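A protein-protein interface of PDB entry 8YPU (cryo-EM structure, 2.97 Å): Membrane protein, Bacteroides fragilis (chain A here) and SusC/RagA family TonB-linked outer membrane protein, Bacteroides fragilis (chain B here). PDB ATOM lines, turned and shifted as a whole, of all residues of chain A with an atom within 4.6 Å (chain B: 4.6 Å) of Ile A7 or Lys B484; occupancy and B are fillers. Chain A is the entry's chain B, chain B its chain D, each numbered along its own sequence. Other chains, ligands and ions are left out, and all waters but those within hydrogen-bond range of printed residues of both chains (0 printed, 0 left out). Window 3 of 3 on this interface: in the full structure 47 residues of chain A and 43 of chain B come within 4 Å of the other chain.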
ATOM      1  N   ASP A   2     -27.602   5.827  18.032  1.00  0.00           N
ATOM      2  CA  ASP A   2     -26.271   5.302  18.439  1.00  0.00           C
ATOM      3  C   ASP A   2     -25.591   6.299  19.384  1.00  0.00           C
ATOM      4  O   ASP A   2     -25.771   7.518  19.190  1.00  0.00           O
ATOM      5  CB  ASP A   2     -25.397   4.990  17.221  1.00  0.00           C
ATOM      6  CG  ASP A   2     -25.662   3.619  16.624  1.00  0.00           C
ATOM      7  OD1 ASP A   2     -25.116   2.632  17.157  1.00  0.00           O
ATOM      8  OD2 ASP A   2     -26.412   3.549  15.630  1.00  0.00           O
ATOM      9  N   TYR A   4     -22.351   6.003  22.920  1.00  0.00           N
ATOM     10  CA  TYR A   4     -21.043   5.434  23.341  1.00  0.00           C
ATOM     11  C   TYR A   4     -20.062   6.042  22.332  1.00  0.00           C
ATOM     12  O   TYR A   4     -19.492   5.289  21.517  1.00  0.00           O
ATOM     13  CB  TYR A   4     -21.067   3.906  23.239  1.00  0.00           C
ATOM     14  CG  TYR A   4     -20.681   3.183  24.504  1.00  0.00           C
ATOM     15  CD1 TYR A   4     -21.026   3.683  25.749  1.00  0.00           C
ATOM     16  CD2 TYR A   4     -19.968   1.996  24.461  1.00  0.00           C
ATOM     17  CE1 TYR A   4     -20.675   3.025  26.916  1.00  0.00           C
ATOM     18  CE2 TYR A   4     -19.609   1.325  25.618  1.00  0.00           C
ATOM     19  CZ  TYR A   4     -19.964   1.841  26.851  1.00  0.00           C
ATOM     20  OH  TYR A   4     -19.613   1.186  27.996  1.00  0.00           O
ATOM     21  N   LEU A   5     -19.877   7.364  22.392  1.00  0.00           N
ATOM     22  CA  LEU A   5     -18.837   8.067  21.593  1.00  0.00           C
ATOM     23  C   LEU A   5     -17.455   7.741  22.170  1.00  0.00           C
ATOM     24  O   LEU A   5     -16.999   8.480  23.065  1.00  0.00           O
ATOM     25  CB  LEU A   5     -19.110   9.573  21.634  1.00  0.00           C
ATOM     26  CG  LEU A   5     -19.931  10.060  22.826  1.00  0.00           C
ATOM     27  CD1 LEU A   5     -19.040  10.737  23.857  1.00  0.00           C
ATOM     28  CD2 LEU A   5     -21.036  11.003  22.376  1.00  0.00           C
ATOM     29  N   ASP A   6     -16.823   6.674  21.670  1.00  0.00           N
ATOM     30  CA  ASP A   6     -15.477   6.256  22.150  1.00  0.00           C
ATOM     31  C   ASP A   6     -14.783   5.436  21.057  1.00  0.00           C
ATOM     32  O   ASP A   6     -13.823   4.710  21.383  1.00  0.00           O
ATOM     33  CB  ASP A   6     -15.571   5.480  23.467  1.00  0.00           C
ATOM     34  CG  ASP A   6     -14.344   5.637  24.348  1.00  0.00           C
ATOM     35  OD1 ASP A   6     -13.228   5.404  23.842  1.00  0.00           O
ATOM     36  OD2 ASP A   6     -14.515   5.989  25.531  1.00  0.00           O
ATOM     37  N   ILE A   7     -15.258   5.555  19.813  1.00  0.00           N
ATOM     38  CA  ILE A   7     -14.666   4.808  18.662  1.00  0.00           C
ATOM     39  C   ILE A   7     -13.253   5.345  18.402  1.00  0.00           C
ATOM     40  O   ILE A   7     -13.129   6.534  18.048  1.00  0.00           O
ATOM     41  CB  ILE A   7     -15.563   4.924  17.413  1.00  0.00           C
ATOM     42  CG1 ILE A   7     -17.049   4.881  17.777  1.00  0.00           C
ATOM     43  CG2 ILE A   7     -15.202   3.861  16.388  1.00  0.00           C
ATOM     44  CD1 ILE A   7     -17.788   6.168  17.497  1.00  0.00           C
ATOM     45  N   ARG A   8     -12.237   4.493  18.572  1.00  0.00           N
ATOM     46  CA  ARG A   8     -10.821   4.893  18.352  1.00  0.00           C
ATOM     47  C   ARG A   8     -10.486   4.772  16.861  1.00  0.00           C
ATOM     48  O   ARG A   8     -11.300   4.189  16.117  1.00  0.00           O
ATOM     49  CB  ARG A   8      -9.885   4.025  19.197  1.00  0.00           C
ATOM     50  CG  ARG A   8     -10.169   4.075  20.691  1.00  0.00           C
ATOM     51  CD  ARG A   8      -9.849   2.765  21.387  1.00  0.00           C
ATOM     52  NE  ARG A   8      -8.881   1.964  20.651  1.00  0.00           N
ATOM     53  CZ  ARG A   8      -7.662   1.667  21.087  1.00  0.00           C
ATOM     54  NH1 ARG A   8      -7.255   2.109  22.264  1.00  0.00           N
ATOM     55  NH2 ARG A   8      -6.855   0.931  20.344  1.00  0.00           N
ATOM     56  N   PRO A   9      -9.328   5.290  16.393  1.00  0.00           N
ATOM     57  CA  PRO A   9      -8.952   5.202  14.979  1.00  0.00           C
ATOM     58  C   PRO A   9      -8.591   3.761  14.589  1.00  0.00           C
ATOM     59  O   PRO A   9      -8.173   3.011  15.452  1.00  0.00           O
ATOM     60  CB  PRO A   9      -7.715   6.106  14.882  1.00  0.00           C
ATOM     61  CG  PRO A   9      -7.122   6.068  16.272  1.00  0.00           C
ATOM     62  CD  PRO A   9      -8.317   5.980  17.199  1.00  0.00           C
ATOM     63  N   SER B 454     -22.479   6.158   5.385  1.00  0.00           N
ATOM     64  CA  SER B 454     -23.703   5.868   6.114  1.00  0.00           C
ATOM     65  C   SER B 454     -23.827   6.819   7.291  1.00  0.00           C
ATOM     66  O   SER B 454     -22.828   7.287   7.837  1.00  0.00           O
ATOM     67  CB  SER B 454     -23.727   4.424   6.617  1.00  0.00           C
ATOM     68  OG  SER B 454     -23.560   3.506   5.557  1.00  0.00           O
ATOM     69  N   GLN B 455     -25.064   7.094   7.687  1.00  0.00           N
ATOM     70  CA  GLN B 455     -25.325   7.971   8.815  1.00  0.00           C
ATOM     71  C   GLN B 455     -26.666   7.618   9.430  1.00  0.00           C
ATOM     72  O   GLN B 455     -27.626   7.342   8.712  1.00  0.00           O
ATOM     73  CB  GLN B 455     -25.312   9.435   8.383  1.00  0.00           C
ATOM     74  CG  GLN B 455     -24.953  10.416   9.469  1.00  0.00           C
ATOM     75  CD  GLN B 455     -25.611  11.752   9.254  1.00  0.00           C
ATOM     76  OE1 GLN B 455     -26.750  11.828   8.809  1.00  0.00           O
ATOM     77  NE2 GLN B 455     -24.895  12.815   9.560  1.00  0.00           N
ATOM     78  N   ILE B 456     -26.726   7.610  10.755  1.00  0.00           N
ATOM     79  CA  ILE B 456     -27.991   7.499  11.470  1.00  0.00           C
ATOM     80  C   ILE B 456     -28.025   8.586  12.530  1.00  0.00           C
ATOM     81  O   ILE B 456     -27.137   8.654  13.385  1.00  0.00           O
ATOM     82  CB  ILE B 456     -28.199   6.108  12.095  1.00  0.00           C
ATOM     83  CG1 ILE B 456     -29.421   6.110  13.007  1.00  0.00           C
ATOM     84  CG2 ILE B 456     -26.980   5.656  12.861  1.00  0.00           C
ATOM     85  CD1 ILE B 456     -29.850   4.739  13.428  1.00  0.00           C
ATOM     86  N   LEU B 482     -28.437  12.123  19.036  1.00  0.00           N
ATOM     87  CA  LEU B 482     -27.345  11.172  18.876  1.00  0.00           C
ATOM     88  C   LEU B 482     -27.158  10.891  17.396  1.00  0.00           C
ATOM     89  O   LEU B 482     -28.109  10.517  16.711  1.00  0.00           O
ATOM     90  CB  LEU B 482     -27.613   9.857  19.611  1.00  0.00           C
ATOM     91  CG  LEU B 482     -28.194   9.840  21.018  1.00  0.00           C
ATOM     92  CD1 LEU B 482     -28.886   8.524  21.236  1.00  0.00           C
ATOM     93  CD2 LEU B 482     -27.100  10.020  22.037  1.00  0.00           C
ATOM     94  N   ARG B 483     -25.937  11.047  16.906  1.00  0.00           N
ATOM     95  CA  ARG B 483     -25.678  10.891  15.482  1.00  0.00           C
ATOM     96  C   ARG B 483     -24.403  10.097  15.271  1.00  0.00           C
ATOM     97  O   ARG B 483     -23.351  10.472  15.782  1.00  0.00           O
ATOM     98  CB  ARG B 483     -25.582  12.251  14.800  1.00  0.00           C
ATOM     99  CG  ARG B 483     -25.146  12.178  13.374  1.00  0.00           C
ATOM    100  CD  ARG B 483     -25.287  13.516  12.729  1.00  0.00           C
ATOM    101  NE  ARG B 483     -24.348  14.473  13.291  1.00  0.00           N
ATOM    102  CZ  ARG B 483     -23.099  14.621  12.881  1.00  0.00           C
ATOM    103  NH1 ARG B 483     -22.590  13.861  11.930  1.00  0.00           N
ATOM    104  NH2 ARG B 483     -22.340  15.551  13.446  1.00  0.00           N
ATOM    105  N   LYS B 484     -24.486   9.017  14.507  1.00  0.00           N
ATOM    106  CA  LYS B 484     -23.328   8.196  14.196  1.00  0.00           C
ATOM    107  C   LYS B 484     -23.130   8.139  12.691  1.00  0.00           C
ATOM    108  O   LYS B 484     -24.097   8.112  11.927  1.00  0.00           O
ATOM    109  CB  LYS B 484     -23.471   6.788  14.770  1.00  0.00           C
ATOM    110  CG  LYS B 484     -22.140   6.133  15.111  1.00  0.00           C
ATOM    111  CD  LYS B 484     -22.305   4.985  16.077  1.00  0.00           C
ATOM    112  CE  LYS B 484     -20.981   4.522  16.625  1.00  0.00           C
ATOM    113  NZ  LYS B 484     -20.065   4.103  15.539  1.00  0.00           N
ATOM    114  N   THR B 485     -21.869   8.131  12.275  1.00  0.00           N
ATOM    115  CA  THR B 485     -21.491   8.194  10.874  1.00  0.00           C
ATOM    116  C   THR B 485     -20.414   7.163  10.584  1.00  0.00           C
ATOM    117  O   THR B 485     -19.497   6.974  11.385  1.00  0.00           O
ATOM    118  CB  THR B 485     -20.975   9.585  10.504  1.00  0.00           C
ATOM    119  OG1 THR B 485     -21.690  10.576  11.246  1.00  0.00           O
ATOM    120  CG2 THR B 485     -21.170   9.844   9.031  1.00  0.00           C
ATOM    121  N   TRP B 486     -20.527   6.507   9.430  1.00  0.00           N
ATOM    122  CA  TRP B 486     -19.534   5.563   8.938  1.00  0.00           C
ATOM    123  C   TRP B 486     -19.092   5.979   7.547  1.00  0.00           C
ATOM    124  O   TRP B 486     -19.910   6.409   6.731  1.00  0.00           O
ATOM    125  CB  TRP B 486     -20.086   4.136   8.875  1.00  0.00           C
ATOM    126  CG  TRP B 486     -20.586   3.614  10.167  1.00  0.00           C
ATOM    127  CD1 TRP B 486     -19.900   2.860  11.057  1.00  0.00           C
ATOM    128  CD2 TRP B 486     -21.893   3.797  10.716  1.00  0.00           C
ATOM    129  NE1 TRP B 486     -20.688   2.568  12.137  1.00  0.00           N
ATOM    130  CE2 TRP B 486     -21.919   3.132  11.951  1.00  0.00           C
ATOM    131  CE3 TRP B 486     -23.040   4.461  10.285  1.00  0.00           C
ATOM    132  CZ2 TRP B 486     -23.044   3.110  12.757  1.00  0.00           C
ATOM    133  CZ3 TRP B 486     -24.150   4.436  11.084  1.00  0.00           C
ATOM    134  CH2 TRP B 486     -24.147   3.769  12.305  1.00  0.00           C
ATOM    135  N   GLU B 527     -15.366   5.622  11.788  1.00  0.00           N
ATOM    136  CA  GLU B 527     -16.589   5.799  12.560  1.00  0.00           C
ATOM    137  C   GLU B 527     -16.518   7.093  13.345  1.00  0.00           C
ATOM    138  O   GLU B 527     -15.441   7.522  13.764  1.00  0.00           O
ATOM    139  CB  GLU B 527     -16.816   4.688  13.569  1.00  0.00           C
ATOM    140  CG  GLU B 527     -17.325   3.402  13.040  1.00  0.00           C
ATOM    141  CD  GLU B 527     -17.774   2.489  14.154  1.00  0.00           C
ATOM    142  OE1 GLU B 527     -18.005   2.994  15.269  1.00  0.00           O
ATOM    143  OE2 GLU B 527     -17.871   1.267  13.929  1.00  0.00           O
ATOM    144  N   ASN B 528     -17.676   7.699  13.569  1.00  0.00           N
ATOM    145  CA  ASN B 528     -17.745   8.870  14.428  1.00  0.00           C
ATOM    146  C   ASN B 528     -19.097   8.886  15.114  1.00  0.00           C
ATOM    147  O   ASN B 528     -20.102   8.518  14.513  1.00  0.00           O
ATOM    148  CB  ASN B 528     -17.529  10.156  13.632  1.00  0.00           C
ATOM    149  CG  ASN B 528     -16.098  10.322  13.175  1.00  0.00           C
ATOM    150  OD1 ASN B 528     -15.835  10.617  12.013  1.00  0.00           O
ATOM    151  ND2 ASN B 528     -15.163  10.125  14.089  1.00  0.00           N
ATOM    152  N   ALA B 529     -19.114   9.295  16.376  1.00  0.00           N
ATOM    153  CA  ALA B 529     -20.343   9.391  17.145  1.00  0.00           C
ATOM    154  C   ALA B 529     -20.406  10.749  17.819  1.00  0.00           C
ATOM    155  O   ALA B 529     -19.387  11.274  18.270  1.00  0.00           O
ATOM    156  CB  ALA B 529     -20.444   8.286  18.186  1.00  0.00           C
ATOM    157  N   ASP B 557     -16.308  11.655  19.594  1.00  0.00           N
ATOM    158  CA  ASP B 557     -15.101  10.855  19.709  1.00  0.00           C
ATOM    159  C   ASP B 557     -13.895  11.526  19.069  1.00  0.00           C
ATOM    160  O   ASP B 557     -12.774  11.038  19.229  1.00  0.00           O
ATOM    161  CB  ASP B 557     -15.323   9.478  19.082  1.00  0.00           C
ATOM    162  CG  ASP B 557     -15.375   9.532  17.579  1.00  0.00           C
ATOM    163  OD1 ASP B 557     -16.168  10.328  17.043  1.00  0.00           O
ATOM    164  OD2 ASP B 557     -14.622   8.779  16.930  1.00  0.00           O
ATOM    165  N   PHE B 614      -5.841  10.702  19.854  1.00  0.00           N
ATOM    166  CA  PHE B 614      -5.251   9.432  20.232  1.00  0.00           C
ATOM    167  C   PHE B 614      -3.780   9.392  19.859  1.00  0.00           C
ATOM    168  O   PHE B 614      -3.308  10.147  19.007  1.00  0.00           O
ATOM    169  CB  PHE B 614      -5.984   8.269  19.559  1.00  0.00           C
ATOM    170  CG  PHE B 614      -7.369   8.048  20.074  1.00  0.00           C
ATOM    171  CD1 PHE B 614      -7.577   7.434  21.289  1.00  0.00           C
ATOM    172  CD2 PHE B 614      -8.464   8.444  19.339  1.00  0.00           C
ATOM    173  CE1 PHE B 614      -8.849   7.229  21.761  1.00  0.00           C
ATOM    174  CE2 PHE B 614      -9.735   8.244  19.811  1.00  0.00           C
ATOM    175  CZ  PHE B 614      -9.926   7.633  21.020  1.00  0.00           C
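The backbone carbonyl oxygen (O) of Ile A7 lies close to the side-chain carboxylate (OD2) of Asp B557 (2.9 Å).
Printed residues of chain B within 4 Å of Leu A5: Ala B529. Ile A7 touches five residues of chain B. Of the printed residues of chain A, Leu B482 touches Asp A2. Lys B484 touches just these residues of chain A: Asp A2 and Ile A7. Thr B485 touches none of the printed residues of chain A. Printed residues of chain A within 4 Å of Asp B557: Ile A7. The nearest residue of chain B that does not touch Ile A7 is Phe B614 (4.2 Å).
Asp A2 touches Ile B456. Leu B482 touches Asp A2. Asp A2 touches Lys B484 (CB to CD, 3.3 Å). CA of Leu A5 touches CB of Ala B529 (3.8 Å). Lys B484 touches Ile A7 (NZ to CD1, 3.6 Å). CG2 of Ile A7 touches OE1 of Glu B527 (3.1 Å). Ile A7 touches Asn B528 (CD1 to C, 3.8 Å). Ile A7 touches Ala B529. Phe B614 touches Arg A8 (CZ to CG, 3.6 Å). Phe B614 touches Pro A9 (CD2 to CD, 3.3 Å).
The backbone carbonyl oxygen of Ile B456 lies within hydrogen-bond range of the backbone NH of Lys B484, at 2.9 Å. NZ of Lys B484 is in salt-bridge range of OE2 of Glu B527 (3.9 Å). O of Asn B528 sits at hydrogen-bond distance from N of Thr B485 (2.9 Å). ND2 of Asn B528 lies within hydrogen-bond range of OD1 of Asp B557 (3.1 Å). The side-chain carboxylate of Asp B557 sits at hydrogen-bond distance from the backbone NH of Ala B529 (3.2 Å).
Printed residues of chain B that touch a printed residue of chain A: Ile B456, Leu B482, Lys B484, Glu B527, Asn B528, Ala B529, Asp B557 and Phe B614. Of the 7 printed residues of chain A, 5 touch a printed residue of chain B. Among the printed residues, 11 pairs touch across the chains. Among the printed residues, no Asp or Glu carboxylate lies within 4 Å of a Lys or Arg side-chain nitrogen of the other chain.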
